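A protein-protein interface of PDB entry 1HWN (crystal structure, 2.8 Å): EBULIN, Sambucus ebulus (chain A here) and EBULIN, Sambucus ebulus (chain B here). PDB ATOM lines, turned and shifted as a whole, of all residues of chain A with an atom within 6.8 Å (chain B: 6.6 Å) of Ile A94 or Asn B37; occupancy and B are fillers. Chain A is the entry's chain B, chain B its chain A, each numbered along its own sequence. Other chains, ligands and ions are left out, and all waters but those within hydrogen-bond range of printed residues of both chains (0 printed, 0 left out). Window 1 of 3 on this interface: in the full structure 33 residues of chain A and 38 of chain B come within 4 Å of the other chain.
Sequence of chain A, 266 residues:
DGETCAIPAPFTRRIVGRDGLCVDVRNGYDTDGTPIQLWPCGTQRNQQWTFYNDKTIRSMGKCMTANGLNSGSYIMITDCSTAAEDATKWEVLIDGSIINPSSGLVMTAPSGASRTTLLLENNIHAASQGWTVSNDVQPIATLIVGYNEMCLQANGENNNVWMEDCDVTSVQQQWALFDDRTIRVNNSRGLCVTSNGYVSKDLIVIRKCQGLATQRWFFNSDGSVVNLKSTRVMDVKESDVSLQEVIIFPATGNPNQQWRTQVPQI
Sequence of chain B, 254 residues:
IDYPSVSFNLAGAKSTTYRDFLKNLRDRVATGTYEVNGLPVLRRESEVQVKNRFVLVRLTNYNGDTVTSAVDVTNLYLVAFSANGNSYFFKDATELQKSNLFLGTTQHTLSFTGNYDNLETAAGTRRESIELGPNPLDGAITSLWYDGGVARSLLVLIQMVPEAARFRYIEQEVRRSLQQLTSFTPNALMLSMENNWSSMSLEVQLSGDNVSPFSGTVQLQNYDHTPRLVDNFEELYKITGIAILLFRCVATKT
The backbone carbonyl oxygen of Asn B37 lies close to the side-chain hydroxyl of Ser A221 (3.5 Å). The backbone carbonyl oxygen of Ile A94 sits close to the side-chain carboxylate of Glu B234, at 3.2 Å. The guanidinium group (NH2) of Arg A181 lies within salt-bridge range of the side-chain carboxylate (OE2) of Glu B234, 2.8 Å away. The backbone carbonyl oxygen (O) of Val A92 is in hydrogen-bond range of the backbone NH (N) of Ser B212 (3.3 Å). O of Val A92 sits close to O of Asn B210 (3.5 Å). The backbone NH (N) of Ile A94 is in hydrogen-bond range of the backbone carbonyl oxygen (O) of Asn B210 (2.8 Å). The backbone NH (N) of Leu B39 sits close to the side-chain hydroxyl (OG) of Ser A221 (3.4 Å).
The side-chain amide nitrogen of Asn B210 lies within hydrogen-bond range of the side-chain carboxylate of Asp B209, at 3.1 Å. The backbone carbonyl oxygen (O) of Ile A94 is in hydrogen-bond range of the guanidinium group (NH1) of Arg A181, 2.8 Å away. O of Ser B212 sits at hydrogen-bond distance from N of Phe B233 (2.9 Å). The backbone NH of Asn B37 sits at hydrogen-bond distance from the side-chain carboxylate of Asp B209 (2.9 Å). The backbone NH (N) of Asn B210 sits at hydrogen-bond distance from the side-chain amide oxygen (OD1) of Asn B37 (2.9 Å). The side-chain hydroxyl (OG) of Ser B212 is in hydrogen-bond range of the side-chain carboxylate (OE1) of Glu B234 (3.2 Å).
Val B211 touches Val A92. CD of Pro B213 touches CG1 of Val A92 (3.6 Å). Leu A93 touches Asn B210 (CA to O, 3.2 Å). CB of Ser B212 touches O of Leu A93, 3.8 Å away. Ile A94 touches Asn B37. Ser B212 touches Ile A94. Ser A221 touches Gly B38.
Asn B37 touches just these residues of chain A: Ile A94 (3.0 Å) and Ser A221 (3.2 Å). Of the printed residues of chain B, Arg A181 touches Glu B234. Of the printed residues of chain A, Asn B210 touches Val A92, Leu A93 and Ile A94. Printed residues of chain A within 4 Å of Gly B38: Ser A221 (3.5 Å). Of the printed residues of chain A, Leu B39 touches Ser A221 (3.3 Å). Of the printed residues of chain B, Leu A93 touches Asn B210 and Ser B212. Val B36 touches none of the printed residues of chain A. The nearest printed residue of chain A that does not touch Glu B234 is Leu A93 (4.03 Å).
Of the 13 printed residues of chain A, 5 touch a printed residue of chain B. Printed residues of chain A that touch a printed residue of chain B: Val A92, Leu A93, Ile A94, Arg A181 and Ser A221. Along chain A the printed residues that touch a printed residue of chain B span positions 92 to 221. Of the 14 printed residues of chain B, 8 touch a printed residue of chain A. Printed residues of chain B that touch a printed residue of chain A: Asn B37, Gly B38, Leu B39, Asn B210, Val B211, Ser B212, Pro B213 and Glu B234. Hydrophobic or aromatic side chains of chain B within 4 Å of the printed part of chain A: Leu B39 and Pro B213.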
ATOM      1  N   VAL A  92       4.017 -12.759 -17.438  1.00  0.00           N
ATOM      2  CA  VAL A  92       3.679 -11.496 -16.789  1.00  0.00           C
ATOM      3  C   VAL A  92       2.205 -11.148 -16.971  1.00  0.00           C
ATOM      4  O   VAL A  92       1.832 -10.455 -17.919  1.00  0.00           O
ATOM      5  CB  VAL A  92       4.527 -10.338 -17.354  1.00  0.00           C
ATOM      6  CG1 VAL A  92       4.313  -9.082 -16.526  1.00  0.00           C
ATOM      7  CG2 VAL A  92       5.993 -10.728 -17.367  1.00  0.00           C
ATOM      8  N   LEU A  93       1.371 -11.624 -16.053  1.00  0.00           N
ATOM      9  CA  LEU A  93      -0.064 -11.369 -16.111  1.00  0.00           C
ATOM     10  C   LEU A  93      -0.380  -9.912 -15.793  1.00  0.00           C
ATOM     11  O   LEU A  93       0.465  -9.179 -15.280  1.00  0.00           O
ATOM     12  CB  LEU A  93      -0.800 -12.280 -15.126  1.00  0.00           C
ATOM     13  CG  LEU A  93      -0.612 -13.789 -15.310  1.00  0.00           C
ATOM     14  CD1 LEU A  93      -1.612 -14.534 -14.440  1.00  0.00           C
ATOM     15  CD2 LEU A  93      -0.793 -14.162 -16.775  1.00  0.00           C
ATOM     16  N   ILE A  94      -1.608  -9.501 -16.095  1.00  0.00           N
ATOM     17  CA  ILE A  94      -2.032  -8.131 -15.843  1.00  0.00           C
ATOM     18  C   ILE A  94      -2.298  -7.898 -14.359  1.00  0.00           C
ATOM     19  O   ILE A  94      -2.593  -6.776 -13.942  1.00  0.00           O
ATOM     20  CB  ILE A  94      -3.306  -7.782 -16.641  1.00  0.00           C
ATOM     21  CG1 ILE A  94      -4.330  -8.912 -16.521  1.00  0.00           C
ATOM     22  CG2 ILE A  94      -2.952  -7.542 -18.097  1.00  0.00           C
ATOM     23  CD1 ILE A  94      -5.727  -8.515 -16.951  1.00  0.00           C
ATOM     24  N   ASP A  95      -2.196  -8.958 -13.564  1.00  0.00           N
ATOM     25  CA  ASP A  95      -2.414  -8.851 -12.125  1.00  0.00           C
ATOM     26  C   ASP A  95      -1.117  -8.450 -11.443  1.00  0.00           C
ATOM     27  O   ASP A  95      -1.058  -8.344 -10.219  1.00  0.00           O
ATOM     28  CB  ASP A  95      -2.883 -10.184 -11.542  1.00  0.00           C
ATOM     29  CG  ASP A  95      -3.796 -10.943 -12.476  1.00  0.00           C
ATOM     30  OD1 ASP A  95      -3.936 -12.169 -12.293  1.00  0.00           O
ATOM     31  OD2 ASP A  95      -4.373 -10.314 -13.390  1.00  0.00           O
ATOM     32  N   GLY A  96      -0.077  -8.233 -12.240  1.00  0.00           N
ATOM     33  CA  GLY A  96       1.208  -7.855 -11.685  1.00  0.00           C
ATOM     34  C   GLY A  96       1.894  -9.034 -11.022  1.00  0.00           C
ATOM     35  O   GLY A  96       2.782  -8.862 -10.188  1.00  0.00           O
ATOM     36  N   SER A  97       1.476 -10.239 -11.398  1.00  0.00           N
ATOM     37  CA  SER A  97       2.044 -11.458 -10.836  1.00  0.00           C
ATOM     38  C   SER A  97       2.918 -12.184 -11.850  1.00  0.00           C
ATOM     39  O   SER A  97       2.424 -12.676 -12.866  1.00  0.00           O
ATOM     40  CB  SER A  97       0.926 -12.397 -10.372  1.00  0.00           C
ATOM     41  OG  SER A  97       0.725 -12.306  -8.972  1.00  0.00           O
ATOM     42  N   ARG A 181       1.366  -3.000  -7.238  1.00  0.00           N
ATOM     43  CA  ARG A 181      -0.088  -3.108  -7.201  1.00  0.00           C
ATOM     44  C   ARG A 181      -0.677  -2.680  -5.859  1.00  0.00           C
ATOM     45  O   ARG A 181      -1.696  -3.216  -5.418  1.00  0.00           O
ATOM     46  CB  ARG A 181      -0.525  -4.541  -7.529  1.00  0.00           C
ATOM     47  CG  ARG A 181      -0.202  -4.992  -8.955  1.00  0.00           C
ATOM     48  CD  ARG A 181      -0.150  -3.818  -9.927  1.00  0.00           C
ATOM     49  NE  ARG A 181       0.703  -4.093 -11.079  1.00  0.00           N
ATOM     50  CZ  ARG A 181       0.311  -4.778 -12.150  1.00  0.00           C
ATOM     51  NH1 ARG A 181      -0.924  -5.256 -12.215  1.00  0.00           N
ATOM     52  NH2 ARG A 181       1.149  -4.981 -13.156  1.00  0.00           N
ATOM     53  N   ARG A 216      -3.616  -5.685  -2.105  1.00  0.00           N
ATOM     54  CA  ARG A 216      -3.461  -5.960  -3.529  1.00  0.00           C
ATOM     55  C   ARG A 216      -4.658  -5.378  -4.271  1.00  0.00           C
ATOM     56  O   ARG A 216      -5.804  -5.718  -3.973  1.00  0.00           O
ATOM     57  CB  ARG A 216      -3.391  -7.470  -3.784  1.00  0.00           C
ATOM     58  CG  ARG A 216      -2.027  -7.979  -4.246  1.00  0.00           C
ATOM     59  CD  ARG A 216      -1.494  -7.199  -5.446  1.00  0.00           C
ATOM     60  NE  ARG A 216      -1.521  -7.975  -6.689  1.00  0.00           N
ATOM     61  CZ  ARG A 216      -0.859  -9.114  -6.884  1.00  0.00           C
ATOM     62  NH1 ARG A 216      -0.947  -9.744  -8.047  1.00  0.00           N
ATOM     63  NH2 ARG A 216      -0.109  -9.624  -5.918  1.00  0.00           N
ATOM     64  N   PHE A 218      -6.180  -4.593  -8.200  1.00  0.00           N
ATOM     65  CA  PHE A 218      -6.096  -4.760  -9.642  1.00  0.00           C
ATOM     66  C   PHE A 218      -7.185  -3.917 -10.299  1.00  0.00           C
ATOM     67  O   PHE A 218      -8.371  -4.239 -10.212  1.00  0.00           O
ATOM     68  CB  PHE A 218      -6.272  -6.234 -10.015  1.00  0.00           C
ATOM     69  CG  PHE A 218      -6.705  -6.455 -11.436  1.00  0.00           C
ATOM     70  CD1 PHE A 218      -5.845  -6.168 -12.491  1.00  0.00           C
ATOM     71  CD2 PHE A 218      -7.975  -6.943 -11.720  1.00  0.00           C
ATOM     72  CE1 PHE A 218      -6.246  -6.364 -13.812  1.00  0.00           C
ATOM     73  CE2 PHE A 218      -8.386  -7.142 -13.036  1.00  0.00           C
ATOM     74  CZ  PHE A 218      -7.520  -6.851 -14.083  1.00  0.00           C
ATOM     75  N   PHE A 219      -6.773  -2.835 -10.949  1.00  0.00           N
ATOM     76  CA  PHE A 219      -7.707  -1.937 -11.617  1.00  0.00           C
ATOM     77  C   PHE A 219      -8.387  -2.613 -12.805  1.00  0.00           C
ATOM     78  O   PHE A 219      -7.938  -2.483 -13.945  1.00  0.00           O
ATOM     79  CB  PHE A 219      -6.971  -0.677 -12.087  1.00  0.00           C
ATOM     80  CG  PHE A 219      -6.534   0.231 -10.967  1.00  0.00           C
ATOM     81  CD1 PHE A 219      -5.730  -0.249  -9.937  1.00  0.00           C
ATOM     82  CD2 PHE A 219      -6.921   1.567 -10.946  1.00  0.00           C
ATOM     83  CE1 PHE A 219      -5.317   0.588  -8.904  1.00  0.00           C
ATOM     84  CE2 PHE A 219      -6.511   2.413  -9.918  1.00  0.00           C
ATOM     85  CZ  PHE A 219      -5.709   1.921  -8.895  1.00  0.00           C
ATOM     86  N   ASN A 220      -9.473  -3.332 -12.536  1.00  0.00           N
ATOM     87  CA  ASN A 220     -10.205  -4.023 -13.590  1.00  0.00           C
ATOM     88  C   ASN A 220     -10.570  -3.063 -14.720  1.00  0.00           C
ATOM     89  O   ASN A 220     -11.037  -1.951 -14.476  1.00  0.00           O
ATOM     90  CB  ASN A 220     -11.474  -4.657 -13.020  1.00  0.00           C
ATOM     91  CG  ASN A 220     -12.055  -5.717 -13.932  1.00  0.00           C
ATOM     92  OD1 ASN A 220     -12.259  -5.484 -15.123  1.00  0.00           O
ATOM     93  ND2 ASN A 220     -12.324  -6.891 -13.377  1.00  0.00           N
ATOM     94  N   SER A 221     -10.354  -3.502 -15.957  1.00  0.00           N
ATOM     95  CA  SER A 221     -10.646  -2.684 -17.129  1.00  0.00           C
ATOM     96  C   SER A 221     -12.113  -2.269 -17.201  1.00  0.00           C
ATOM     97  O   SER A 221     -12.469  -1.351 -17.941  1.00  0.00           O
ATOM     98  CB  SER A 221     -10.263  -3.441 -18.406  1.00  0.00           C
ATOM     99  OG  SER A 221     -11.336  -3.467 -19.335  1.00  0.00           O
ATOM    100  N   ASP A 222     -12.962  -2.946 -16.436  1.00  0.00           N
ATOM    101  CA  ASP A 222     -14.386  -2.632 -16.426  1.00  0.00           C
ATOM    102  C   ASP A 222     -14.656  -1.368 -15.612  1.00  0.00           C
ATOM    103  O   ASP A 222     -15.773  -0.850 -15.602  1.00  0.00           O
ATOM    104  CB  ASP A 222     -15.188  -3.804 -15.855  1.00  0.00           C
ATOM    105  CG  ASP A 222     -15.106  -3.889 -14.346  1.00  0.00           C
ATOM    106  OD1 ASP A 222     -14.062  -3.503 -13.781  1.00  0.00           O
ATOM    107  OD2 ASP A 222     -16.089  -4.343 -13.722  1.00  0.00           O
ATOM    108  N   GLU B  35     -12.440  -9.927 -27.372  1.00  0.00           N
ATOM    109  CA  GLU B  35     -12.064  -9.101 -26.233  1.00  0.00           C
ATOM    110  C   GLU B  35     -10.570  -9.182 -25.941  1.00  0.00           C
ATOM    111  O   GLU B  35      -9.855  -9.993 -26.527  1.00  0.00           O
ATOM    112  CB  GLU B  35     -12.849  -9.534 -24.994  1.00  0.00           C
ATOM    113  CG  GLU B  35     -14.163  -8.797 -24.805  1.00  0.00           C
ATOM    114  CD  GLU B  35     -14.679  -8.887 -23.383  1.00  0.00           C
ATOM    115  OE1 GLU B  35     -13.993  -9.507 -22.542  1.00  0.00           O
ATOM    116  OE2 GLU B  35     -15.768  -8.337 -23.108  1.00  0.00           O
ATOM    117  N   VAL B  36     -10.109  -8.330 -25.030  1.00  0.00           N
ATOM    118  CA  VAL B  36      -8.702  -8.292 -24.642  1.00  0.00           C
ATOM    119  C   VAL B  36      -8.544  -7.578 -23.303  1.00  0.00           C
ATOM    120  O   VAL B  36      -8.579  -6.348 -23.235  1.00  0.00           O
ATOM    121  CB  VAL B  36      -7.847  -7.559 -25.699  1.00  0.00           C
ATOM    122  CG1 VAL B  36      -7.190  -8.569 -26.626  1.00  0.00           C
ATOM    123  CG2 VAL B  36      -8.712  -6.586 -26.494  1.00  0.00           C
ATOM    124  N   ASN B  37      -8.380  -8.360 -22.240  1.00  0.00           N
ATOM    125  CA  ASN B  37      -8.220  -7.813 -20.895  1.00  0.00           C
ATOM    126  C   ASN B  37      -9.486  -7.087 -20.457  1.00  0.00           C
ATOM    127  O   ASN B  37      -9.492  -6.389 -19.442  1.00  0.00           O
ATOM    128  CB  ASN B  37      -7.031  -6.848 -20.849  1.00  0.00           C
ATOM    129  CG  ASN B  37      -5.702  -7.544 -21.075  1.00  0.00           C
ATOM    130  OD1 ASN B  37      -5.109  -8.090 -20.147  1.00  0.00           O
ATOM    131  ND2 ASN B  37      -5.228  -7.524 -22.314  1.00  0.00           N
ATOM    132  N   GLY B  38     -10.557  -7.257 -21.226  1.00  0.00           N
ATOM    133  CA  GLY B  38     -11.815  -6.612 -20.900  1.00  0.00           C
ATOM    134  C   GLY B  38     -12.313  -5.724 -22.024  1.00  0.00           C
ATOM    135  O   GLY B  38     -13.452  -5.854 -22.473  1.00  0.00           O
ATOM    136  N   LEU B  39     -11.457  -4.821 -22.481  1.00  0.00           N
ATOM    137  CA  LEU B  39     -11.812  -3.910 -23.563  1.00  0.00           C
ATOM    138  C   LEU B  39     -12.081  -4.678 -24.853  1.00  0.00           C
ATOM    139  O   LEU B  39     -11.310  -5.558 -25.231  1.00  0.00           O
ATOM    140  CB  LEU B  39     -10.688  -2.900 -23.785  1.00  0.00           C
ATOM    141  CG  LEU B  39      -9.935  -2.485 -22.520  1.00  0.00           C
ATOM    142  CD1 LEU B  39      -8.554  -1.989 -22.895  1.00  0.00           C
ATOM    143  CD2 LEU B  39     -10.715  -1.407 -21.785  1.00  0.00           C
ATOM    144  N   VAL B 204      -2.036  -3.449 -27.592  1.00  0.00           N
ATOM    145  CA  VAL B 204      -2.865  -4.230 -26.685  1.00  0.00           C
ATOM    146  C   VAL B 204      -3.180  -5.590 -27.300  1.00  0.00           C
ATOM    147  O   VAL B 204      -3.218  -6.606 -26.606  1.00  0.00           O
ATOM    148  CB  VAL B 204      -4.189  -3.504 -26.378  1.00  0.00           C
ATOM    149  CG1 VAL B 204      -5.063  -4.365 -25.475  1.00  0.00           C
ATOM    150  CG2 VAL B 204      -3.904  -2.166 -25.718  1.00  0.00           C
ATOM    151  N   GLY B 208      -1.240  -9.291 -26.504  1.00  0.00           N
ATOM    152  CA  GLY B 208      -2.198 -10.349 -26.249  1.00  0.00           C
ATOM    153  C   GLY B 208      -2.943 -10.157 -24.944  1.00  0.00           C
ATOM    154  O   GLY B 208      -2.588  -9.306 -24.130  1.00  0.00           O
ATOM    155  N   ASP B 209      -3.985 -10.954 -24.743  1.00  0.00           N
ATOM    156  CA  ASP B 209      -4.774 -10.861 -23.528  1.00  0.00           C
ATOM    157  C   ASP B 209      -3.955 -11.284 -22.312  1.00  0.00           C
ATOM    158  O   ASP B 209      -3.072 -12.135 -22.412  1.00  0.00           O
ATOM    159  CB  ASP B 209      -6.018 -11.740 -23.645  1.00  0.00           C
ATOM    160  CG  ASP B 209      -7.109 -11.333 -22.680  1.00  0.00           C
ATOM    161  OD1 ASP B 209      -6.831 -11.253 -21.464  1.00  0.00           O
ATOM    162  OD2 ASP B 209      -8.246 -11.090 -23.138  1.00  0.00           O
ATOM    163  N   ASN B 210      -4.251 -10.673 -21.169  1.00  0.00           N
ATOM    164  CA  ASN B 210      -3.567 -10.976 -19.915  1.00  0.00           C
ATOM    165  C   ASN B 210      -2.112 -10.522 -19.863  1.00  0.00           C
ATOM    166  O   ASN B 210      -1.539 -10.392 -18.782  1.00  0.00           O
ATOM    167  CB  ASN B 210      -3.644 -12.475 -19.620  1.00  0.00           C
ATOM    168  CG  ASN B 210      -4.634 -12.800 -18.520  1.00  0.00           C
ATOM    169  OD1 ASN B 210      -4.251 -13.086 -17.386  1.00  0.00           O
ATOM    170  ND2 ASN B 210      -5.919 -12.752 -18.851  1.00  0.00           N
ATOM    171  N   VAL B 211      -1.513 -10.278 -21.024  1.00  0.00           N
ATOM    172  CA  VAL B 211      -0.123  -9.839 -21.077  1.00  0.00           C
ATOM    173  C   VAL B 211      -0.007  -8.341 -20.802  1.00  0.00           C
ATOM    174  O   VAL B 211      -0.474  -7.517 -21.588  1.00  0.00           O
ATOM    175  CB  VAL B 211       0.504 -10.137 -22.455  1.00  0.00           C
ATOM    176  CG1 VAL B 211       1.975  -9.753 -22.451  1.00  0.00           C
ATOM    177  CG2 VAL B 211       0.339 -11.610 -22.788  1.00  0.00           C
ATOM    178  N   SER B 212       0.624  -7.997 -19.685  1.00  0.00           N
ATOM    179  CA  SER B 212       0.797  -6.602 -19.299  1.00  0.00           C
ATOM    180  C   SER B 212       1.798  -5.825 -20.160  1.00  0.00           C
ATOM    181  O   SER B 212       1.480  -4.752 -20.674  1.00  0.00           O
ATOM    182  CB  SER B 212       1.213  -6.516 -17.826  1.00  0.00           C
ATOM    183  OG  SER B 212       2.385  -5.731 -17.668  1.00  0.00           O
ATOM    184  N   PRO B 213       3.025  -6.352 -20.322  1.00  0.00           N
ATOM    185  CA  PRO B 213       4.047  -5.670 -21.127  1.00  0.00           C
ATOM    186  C   PRO B 213       3.653  -5.435 -22.584  1.00  0.00           C
ATOM    187  O   PRO B 213       2.828  -6.158 -23.144  1.00  0.00           O
ATOM    188  CB  PRO B 213       5.270  -6.584 -21.017  1.00  0.00           C
ATOM    189  CG  PRO B 213       5.010  -7.446 -19.828  1.00  0.00           C
ATOM    190  CD  PRO B 213       3.527  -7.620 -19.765  1.00  0.00           C
ATOM    191  N   PHE B 233      -0.032  -2.280 -20.259  1.00  0.00           N
ATOM    192  CA  PHE B 233      -1.479  -2.125 -20.225  1.00  0.00           C
ATOM    193  C   PHE B 233      -1.949  -1.304 -19.028  1.00  0.00           C
ATOM    194  O   PHE B 233      -2.519  -0.227 -19.195  1.00  0.00           O
ATOM    195  CB  PHE B 233      -2.144  -3.501 -20.198  1.00  0.00           C
ATOM    196  CG  PHE B 233      -3.643  -3.449 -20.245  1.00  0.00           C
ATOM    197  CD1 PHE B 233      -4.304  -3.182 -21.438  1.00  0.00           C
ATOM    198  CD2 PHE B 233      -4.395  -3.685 -19.100  1.00  0.00           C
ATOM    199  CE1 PHE B 233      -5.692  -3.153 -21.491  1.00  0.00           C
ATOM    200  CE2 PHE B 233      -5.786  -3.656 -19.142  1.00  0.00           C
ATOM    201  CZ  PHE B 233      -6.436  -3.390 -20.339  1.00  0.00           C
ATOM    202  N   GLU B 234      -1.713  -1.818 -17.825  1.00  0.00           N
ATOM    203  CA  GLU B 234      -2.122  -1.130 -16.606  1.00  0.00           C
ATOM    204  C   GLU B 234      -1.778   0.355 -16.644  1.00  0.00           C
ATOM    205  O   GLU B 234      -2.662   1.204 -16.546  1.00  0.00           O
ATOM    206  CB  GLU B 234      -1.459  -1.777 -15.387  1.00  0.00           C
ATOM    207  CG  GLU B 234      -1.620  -3.289 -15.321  1.00  0.00           C
ATOM    208  CD  GLU B 234      -0.420  -4.029 -15.880  1.00  0.00           C
ATOM    209  OE1 GLU B 234       0.336  -3.419 -16.667  1.00  0.00           O
ATOM    210  OE2 GLU B 234      -0.237  -5.217 -15.534  1.00  0.00           O
